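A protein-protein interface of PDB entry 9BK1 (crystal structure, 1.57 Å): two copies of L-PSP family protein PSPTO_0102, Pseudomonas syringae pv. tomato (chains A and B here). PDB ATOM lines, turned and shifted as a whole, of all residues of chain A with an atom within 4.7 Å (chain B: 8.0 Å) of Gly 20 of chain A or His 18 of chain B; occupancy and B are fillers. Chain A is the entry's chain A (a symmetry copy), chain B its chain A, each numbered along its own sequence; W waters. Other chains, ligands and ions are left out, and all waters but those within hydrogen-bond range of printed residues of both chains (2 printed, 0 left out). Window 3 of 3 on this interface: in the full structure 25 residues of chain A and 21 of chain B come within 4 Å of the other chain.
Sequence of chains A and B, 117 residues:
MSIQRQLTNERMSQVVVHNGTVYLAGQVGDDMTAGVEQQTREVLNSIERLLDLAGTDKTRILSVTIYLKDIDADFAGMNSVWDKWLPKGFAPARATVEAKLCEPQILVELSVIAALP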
ATOM      1  N   HIS A  18      26.352 -12.951  38.988  1.00  0.00           N
ATOM      2  CA  HIS A  18      24.955 -12.532  39.082  1.00  0.00           C
ATOM      3  C   HIS A  18      24.292 -12.672  37.724  1.00  0.00           C
ATOM      4  O   HIS A  18      24.688 -11.998  36.769  1.00  0.00           O
ATOM      5  CB  HIS A  18      24.831 -11.089  39.574  1.00  0.00           C
ATOM      6  CG  HIS A  18      23.451 -10.529  39.410  1.00  0.00           C
ATOM      7  ND1 HIS A  18      23.173  -9.466  38.582  1.00  0.00           N
ATOM      8  CD2 HIS A  18      22.265 -10.914  39.944  1.00  0.00           C
ATOM      9  CE1 HIS A  18      21.875  -9.207  38.624  1.00  0.00           C
ATOM     10  NE2 HIS A  18      21.304 -10.068  39.448  1.00  0.00           N
ATOM     11  N   ASN A  19      23.287 -13.546  37.640  1.00  0.00           N
ATOM     12  CA  ASN A  19      22.446 -13.649  36.447  1.00  0.00           C
ATOM     13  C   ASN A  19      23.292 -13.727  35.182  1.00  0.00           C
ATOM     14  O   ASN A  19      23.052 -13.027  34.197  1.00  0.00           O
ATOM     15  CB  ASN A  19      21.466 -12.478  36.370  1.00  0.00           C
ATOM     16  CG  ASN A  19      20.329 -12.614  37.361  1.00  0.00           C
ATOM     17  OD1 ASN A  19      20.300 -13.550  38.165  1.00  0.00           O
ATOM     18  ND2 ASN A  19      19.392 -11.670  37.323  1.00  0.00           N
ATOM     19  N   GLY A  20      24.320 -14.568  35.232  1.00  0.00           N
ATOM     20  CA  GLY A  20      25.131 -14.851  34.072  1.00  0.00           C
ATOM     21  C   GLY A  20      26.329 -13.950  33.869  1.00  0.00           C
ATOM     22  O   GLY A  20      27.106 -14.188  32.935  1.00  0.00           O
ATOM     23  N   THR A  21      26.503 -12.925  34.696  1.00  0.00           N
ATOM     24  CA  THR A  21      27.625 -12.000  34.562  1.00  0.00           C
ATOM     25  C   THR A  21      28.593 -12.200  35.721  1.00  0.00           C
ATOM     26  O   THR A  21      28.171 -12.289  36.876  1.00  0.00           O
ATOM     27  CB  THR A  21      27.130 -10.549  34.507  1.00  0.00           C
ATOM     28  OG1 THR A  21      26.202 -10.407  33.423  1.00  0.00           O
ATOM     29  CG2 THR A  21      28.290  -9.600  34.262  1.00  0.00           C
ATOM     30  N   VAL A  22      29.888 -12.276  35.405  1.00  0.00           N
ATOM     31  CA  VAL A  22      30.965 -12.524  36.359  1.00  0.00           C
ATOM     32  C   VAL A  22      31.714 -11.218  36.577  1.00  0.00           C
ATOM     33  O   VAL A  22      32.225 -10.624  35.622  1.00  0.00           O
ATOM     34  CB  VAL A  22      31.926 -13.609  35.848  1.00  0.00           C
ATOM     35  CG1 VAL A  22      33.045 -13.841  36.842  1.00  0.00           C
ATOM     36  CG2 VAL A  22      31.169 -14.901  35.565  1.00  0.00           C
ATOM     37  N   LEU A  62      33.956  -9.903  28.764  1.00  0.00           N
ATOM     38  CA  LEU A  62      33.126  -8.876  28.151  1.00  0.00           C
ATOM     39  C   LEU A  62      33.818  -7.524  28.129  1.00  0.00           C
ATOM     40  O   LEU A  62      33.803  -6.839  27.097  1.00  0.00           O
ATOM     41  CB  LEU A  62      31.783  -8.762  28.886  1.00  0.00           C
ATOM     42  CG  LEU A  62      30.977 -10.054  29.043  1.00  0.00           C
ATOM     43  CD1 LEU A  62      29.744  -9.798  29.889  1.00  0.00           C
ATOM     44  CD2 LEU A  62      30.595 -10.631  27.676  1.00  0.00           C
ATOM     45  N   ALA A 114      33.068 -10.692  32.887  1.00  0.00           N
ATOM     46  CA  ALA A 114      32.970 -11.827  31.968  1.00  0.00           C
ATOM     47  C   ALA A 114      31.550 -12.389  32.002  1.00  0.00           C
ATOM     48  O   ALA A 114      30.700 -11.937  32.766  1.00  0.00           O
ATOM     49  CB  ALA A 114      33.992 -12.924  32.315  1.00  0.00           C
ATOM     50  N   ALA A 115      31.293 -13.392  31.166  1.00  0.00           N
ATOM     51  CA  ALA A 115      29.969 -13.992  31.049  1.00  0.00           C
ATOM     52  C   ALA A 115      30.055 -15.488  31.286  1.00  0.00           C
ATOM     53  O   ALA A 115      31.021 -16.132  30.878  1.00  0.00           O
ATOM     54  CB  ALA A 115      29.369 -13.727  29.665  1.00  0.00           C
ATOM     55  N   LEU A 116      29.046 -16.040  31.955  1.00  0.00           N
ATOM     56  CA  LEU A 116      28.909 -17.488  32.005  1.00  0.00           C
ATOM     57  C   LEU A 116      28.483 -18.021  30.641  1.00  0.00           C
ATOM     58  O   LEU A 116      27.846 -17.311  29.858  1.00  0.00           O
ATOM     59  CB  LEU A 116      27.869 -17.909  33.036  1.00  0.00           C
ATOM     60  CG  LEU A 116      28.160 -17.651  34.507  1.00  0.00           C
ATOM     61  CD1 LEU A 116      27.040 -18.240  35.345  1.00  0.00           C
ATOM     62  CD2 LEU A 116      29.505 -18.228  34.897  1.00  0.00           C
ATOM     63  N   SER B   2      23.984 -15.234  22.702  1.00  0.00           N
ATOM     64  CA  SER B   2      25.107 -15.449  23.611  1.00  0.00           C
ATOM     65  C   SER B   2      25.895 -14.162  23.800  1.00  0.00           C
ATOM     66  O   SER B   2      25.467 -13.242  24.504  1.00  0.00           O
ATOM     67  CB  SER B   2      26.030 -16.554  23.081  1.00  0.00           C
ATOM     68  OG  SER B   2      26.654 -16.183  21.859  1.00  0.00           O
ATOM     69  N   ILE B   3      27.058 -14.116  23.162  1.00  0.00           N
ATOM     70  CA  ILE B   3      27.914 -12.938  23.138  1.00  0.00           C
ATOM     71  C   ILE B   3      28.150 -12.561  21.686  1.00  0.00           C
ATOM     72  O   ILE B   3      28.541 -13.408  20.875  1.00  0.00           O
ATOM     73  CB  ILE B   3      29.254 -13.191  23.846  1.00  0.00           C
ATOM     74  CG1 ILE B   3      29.019 -13.543  25.314  1.00  0.00           C
ATOM     75  CG2 ILE B   3      30.179 -11.985  23.689  1.00  0.00           C
ATOM     76  CD1 ILE B   3      30.209 -14.195  25.951  1.00  0.00           C
ATOM     77  N   GLN B   4      27.907 -11.298  21.357  1.00  0.00           N
ATOM     78  CA  GLN B   4      28.226 -10.764  20.040  1.00  0.00           C
ATOM     79  C   GLN B   4      29.365  -9.771  20.183  1.00  0.00           C
ATOM     80  O   GLN B   4      29.331  -8.920  21.068  1.00  0.00           O
ATOM     81  CB  GLN B   4      27.013 -10.083  19.402  1.00  0.00           C
ATOM     82  CG  GLN B   4      26.031 -11.065  18.790  1.00  0.00           C
ATOM     83  CD  GLN B   4      25.102 -11.647  19.826  1.00  0.00           C
ATOM     84  OE1 GLN B   4      24.938 -12.866  19.926  1.00  0.00           O
ATOM     85  NE2 GLN B   4      24.478 -10.770  20.610  1.00  0.00           N
ATOM     86  N   ARG B   5      30.375  -9.888  19.328  1.00  0.00           N
ATOM     87  CA  ARG B   5      31.493  -8.953  19.315  1.00  0.00           C
ATOM     88  C   ARG B   5      31.556  -8.282  17.954  1.00  0.00           C
ATOM     89  O   ARG B   5      31.342  -8.931  16.926  1.00  0.00           O
ATOM     90  CB  ARG B   5      32.824  -9.651  19.618  1.00  0.00           C
ATOM     91  CG  ARG B   5      32.832 -10.388  20.938  1.00  0.00           C
ATOM     92  CD  ARG B   5      34.109 -11.175  21.146  1.00  0.00           C
ATOM     93  NE  ARG B   5      34.001 -12.116  22.254  1.00  0.00           N
ATOM     94  CZ  ARG B   5      34.223 -11.788  23.521  1.00  0.00           C
ATOM     95  NH1 ARG B   5      34.586 -10.562  23.858  1.00  0.00           N
ATOM     96  NH2 ARG B   5      34.071 -12.707  24.469  1.00  0.00           N
ATOM     97  N   VAL B  15      32.830  -3.220  20.405  1.00  0.00           N
ATOM     98  CA  VAL B  15      31.474  -3.497  20.871  1.00  0.00           C
ATOM     99  C   VAL B  15      31.405  -4.935  21.360  1.00  0.00           C
ATOM    100  O   VAL B  15      31.777  -5.858  20.625  1.00  0.00           O
ATOM    101  CB  VAL B  15      30.435  -3.289  19.754  1.00  0.00           C
ATOM    102  CG1 VAL B  15      29.057  -3.736  20.224  1.00  0.00           C
ATOM    103  CG2 VAL B  15      30.423  -1.836  19.282  1.00  0.00           C
ATOM    104  N   VAL B  16      30.881  -5.139  22.571  1.00  0.00           N
ATOM    105  CA  VAL B  16      30.557  -6.479  23.050  1.00  0.00           C
ATOM    106  C   VAL B  16      29.148  -6.444  23.613  1.00  0.00           C
ATOM    107  O   VAL B  16      28.826  -5.578  24.429  1.00  0.00           O
ATOM    108  CB  VAL B  16      31.557  -6.988  24.110  1.00  0.00           C
ATOM    109  CG1 VAL B  16      31.138  -8.374  24.631  1.00  0.00           C
ATOM    110  CG2 VAL B  16      32.975  -7.039  23.531  1.00  0.00           C
ATOM    111  N   VAL B  17      28.298  -7.364  23.173  1.00  0.00           N
ATOM    112  CA  VAL B  17      26.907  -7.416  23.601  1.00  0.00           C
ATOM    113  C   VAL B  17      26.676  -8.766  24.262  1.00  0.00           C
ATOM    114  O   VAL B  17      27.001  -9.811  23.682  1.00  0.00           O
ATOM    115  CB  VAL B  17      25.938  -7.194  22.421  1.00  0.00           C
ATOM    116  CG1 VAL B  17      24.484  -7.175  22.901  1.00  0.00           C
ATOM    117  CG2 VAL B  17      26.271  -5.885  21.678  1.00  0.00           C
ATOM    118  N   HIS B  18      26.166  -8.743  25.491  1.00  0.00           N
ATOM    119  CA  HIS B  18      25.901  -9.969  26.241  1.00  0.00           C
ATOM    120  C   HIS B  18      24.563  -9.852  26.948  1.00  0.00           C
ATOM    121  O   HIS B  18      24.397  -8.991  27.816  1.00  0.00           O
ATOM    122  CB  HIS B  18      27.004 -10.258  27.259  1.00  0.00           C
ATOM    123  CG  HIS B  18      26.635 -11.331  28.238  1.00  0.00           C
ATOM    124  ND1 HIS B  18      26.502 -11.095  29.586  1.00  0.00           N
ATOM    125  CD2 HIS B  18      26.334 -12.640  28.050  1.00  0.00           C
ATOM    126  CE1 HIS B  18      26.151 -12.217  30.195  1.00  0.00           C
ATOM    127  NE2 HIS B  18      26.048 -13.170  29.284  1.00  0.00           N
ATOM    128  N   ASN B  19      23.615 -10.714  26.576  1.00  0.00           N
ATOM    129  CA  ASN B  19      22.347 -10.830  27.296  1.00  0.00           C
ATOM    130  C   ASN B  19      21.721  -9.462  27.535  1.00  0.00           C
ATOM    131  O   ASN B  19      21.290  -9.130  28.640  1.00  0.00           O
ATOM    132  CB  ASN B  19      22.539 -11.576  28.616  1.00  0.00           C
ATOM    133  CG  ASN B  19      22.729 -13.064  28.415  1.00  0.00           C
ATOM    134  OD1 ASN B  19      22.790 -13.545  27.280  1.00  0.00           O
ATOM    135  ND2 ASN B  19      22.842 -13.803  29.515  1.00  0.00           N
ATOM    136  N   GLY B  20      21.710  -8.646  26.486  1.00  0.00           N
ATOM    137  CA  GLY B  20      21.035  -7.371  26.518  1.00  0.00           C
ATOM    138  C   GLY B  20      21.866  -6.195  26.983  1.00  0.00           C
ATOM    139  O   GLY B  20      21.367  -5.063  26.961  1.00  0.00           O
ATOM    140  N   THR B  21      23.105  -6.419  27.408  1.00  0.00           N
ATOM    141  CA  THR B  21      23.969  -5.342  27.884  1.00  0.00           C
ATOM    142  C   THR B  21      25.097  -5.113  26.886  1.00  0.00           C
ATOM    143  O   THR B  21      25.722  -6.070  26.423  1.00  0.00           O
ATOM    144  CB  THR B  21      24.528  -5.668  29.275  1.00  0.00           C
ATOM    145  OG1 THR B  21      23.438  -5.904  30.177  1.00  0.00           O
ATOM    146  CG2 THR B  21      25.339  -4.502  29.810  1.00  0.00           C
ATOM    147  N   VAL B  22      25.348  -3.844  26.556  1.00  0.00           N
ATOM    148  CA  VAL B  22      26.344  -3.420  25.576  1.00  0.00           C
ATOM    149  C   VAL B  22      27.525  -2.825  26.329  1.00  0.00           C
ATOM    150  O   VAL B  22      27.360  -1.870  27.094  1.00  0.00           O
ATOM    151  CB  VAL B  22      25.762  -2.387  24.599  1.00  0.00           C
ATOM    152  CG1 VAL B  22      26.812  -1.945  23.602  1.00  0.00           C
ATOM    153  CG2 VAL B  22      24.538  -2.954  23.889  1.00  0.00           C
ATOM    154  N   TYR B  23      28.713  -3.382  26.113  1.00  0.00           N
ATOM    155  CA  TYR B  23      29.956  -2.889  26.692  1.00  0.00           C
ATOM    156  C   TYR B  23      30.801  -2.316  25.566  1.00  0.00           C
ATOM    157  O   TYR B  23      31.150  -3.035  24.619  1.00  0.00           O
ATOM    158  CB  TYR B  23      30.721  -4.009  27.398  1.00  0.00           C
ATOM    159  CG  TYR B  23      29.937  -4.690  28.498  1.00  0.00           C
ATOM    160  CD1 TYR B  23      29.082  -5.746  28.223  1.00  0.00           C
ATOM    161  CD2 TYR B  23      30.057  -4.264  29.823  1.00  0.00           C
ATOM    162  CE1 TYR B  23      28.363  -6.353  29.238  1.00  0.00           C
ATOM    163  CE2 TYR B  23      29.355  -4.873  30.833  1.00  0.00           C
ATOM    164  CZ  TYR B  23      28.512  -5.918  30.537  1.00  0.00           C
ATOM    165  OH  TYR B  23      27.800  -6.516  31.551  1.00  0.00           O
ATOM    166  N   ALA B 114      25.664   0.248  28.009  1.00  0.00           N
ATOM    167  CA  ALA B 114      24.328   0.579  27.510  1.00  0.00           C
ATOM    168  C   ALA B 114      23.470  -0.685  27.476  1.00  0.00           C
ATOM    169  O   ALA B 114      23.934  -1.783  27.776  1.00  0.00           O
ATOM    170  CB  ALA B 114      24.391   1.225  26.115  1.00  0.00           C
ATOM    171  N   LEU B 116      20.415  -2.987  25.246  1.00  0.00           N
ATOM    172  CA  LEU B 116      19.600  -3.201  24.059  1.00  0.00           C
ATOM    173  C   LEU B 116      18.138  -2.894  24.368  1.00  0.00           C
ATOM    174  O   LEU B 116      17.699  -3.006  25.515  1.00  0.00           O
ATOM    175  CB  LEU B 116      19.702  -4.640  23.571  1.00  0.00           C
ATOM    176  CG  LEU B 116      21.036  -5.129  23.028  1.00  0.00           C
ATOM    177  CD1 LEU B 116      20.872  -6.547  22.513  1.00  0.00           C
ATOM    178  CD2 LEU B 116      21.546  -4.203  21.945  1.00  0.00           C
HETATM  179  O   HOH W   1      25.568 -15.955  29.862  1.00  0.00           O
HETATM  180  O   HOH W   2      26.349  -8.856  31.209  1.00  0.00           O
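The backbone carbonyl oxygen (O) of Val 16 of chain B lies within hydrogen-bond range of the backbone NH (N) of Tyr 23 of chain B (2.8 Å).
ND2 of Asn 19 of chain B is in hydrogen-bond range of NE2 of His 18 of chain B, 3.3 Å away.
The backbone carbonyl oxygen (O) of Gly 20 of chain A is in hydrogen-bond range of the backbone NH (N) of Leu 116 of chain A (2.9 Å).
O of Gly 20 of chain A touches CE1 of His 18 of chain B, at 3.5 Å.
Thr 21 of chain A touches His 18 of chain B.
CD1 of Ile 3 of chain B touches CD2 of Leu 62 of chain A, 3.98 Å away.
O of Leu 62 of chain A touches CG2 of Val 16 of chain B (3.7 Å).
ND1 of His 18 of chain B touches CD1 of Leu 62 of chain A (3.5 Å).
CD1 of Leu 62 of chain A touches CE1 of Tyr 23 of chain B, 3.8 Å away.
Ala 115 of chain A touches Ile 3 of chain B.
CB of Ala 115 of chain A touches NE2 of His 18 of chain B, at 3.4 Å.
Of the printed residues of chain B, Gly 20 of chain A touches His 18 (3.5 Å).
Printed residues of chain B within 4 Å of Thr 21 of chain A: His 18 (3.7 Å).
Val 22 of chain A touches none of the printed residues of chain B.
Printed residues of chain A within 4 Å of Ile 3 of chain B: Leu 62 (3.98 Å) and Ala 115 (3.8 Å).
Printed residues of chain A within 4 Å of Tyr 23 of chain B: Leu 62 (3.8 Å).
Ala 114 of chain B touches none of the printed residues of chain A.
Of the 9 printed residues of chain A, 4 touch a printed residue of chain B.
Hydrophobic or aromatic side chains of chain A within 4 Å of the printed part of chain B: Leu 62 and Ala 115.
Printed residues of chain B that touch a printed residue of chain A: Ile 3, Val 16, His 18 and Tyr 23.
Hydrophobic or aromatic side chains of chain B within 4 Å of the printed part of chain A: Ile 3, Val 16, His 18 and Tyr 23.
Among the printed residues, no Asp or Glu carboxylate lies within 4 Å of a Lys or Arg side-chain nitrogen of the other chain.
Gly 20 of chain A touches His 18 of chain B, but with the chains exchanged His 18 of chain A does not touch Gly 20 of chain B (11.2 Å).
Thr 21 of chain A touches His 18 of chain B, but with the chains exchanged His 18 of chain A does not touch Thr 21 of chain B (9.1 Å).
Positions printed for both chains: 18, 19, 20, 21, 22, 114 and 116.
Of the 8 pairs that touch across the chains among the printed residues, none has its exchanged pair printed and touching as well.
Water W1 lies within hydrogen-bond range of O of Leu 116 of chain A (2.7 Å), NE2 of His 18 of chain B (2.9 Å) and ND2 of Asn 19 of chain B (3.5 Å).
Water W2 lies within hydrogen-bond range of OG1 of Thr 21 of chain A, ND1 of His 18 of chain B and OH of Tyr 23 of chain B.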
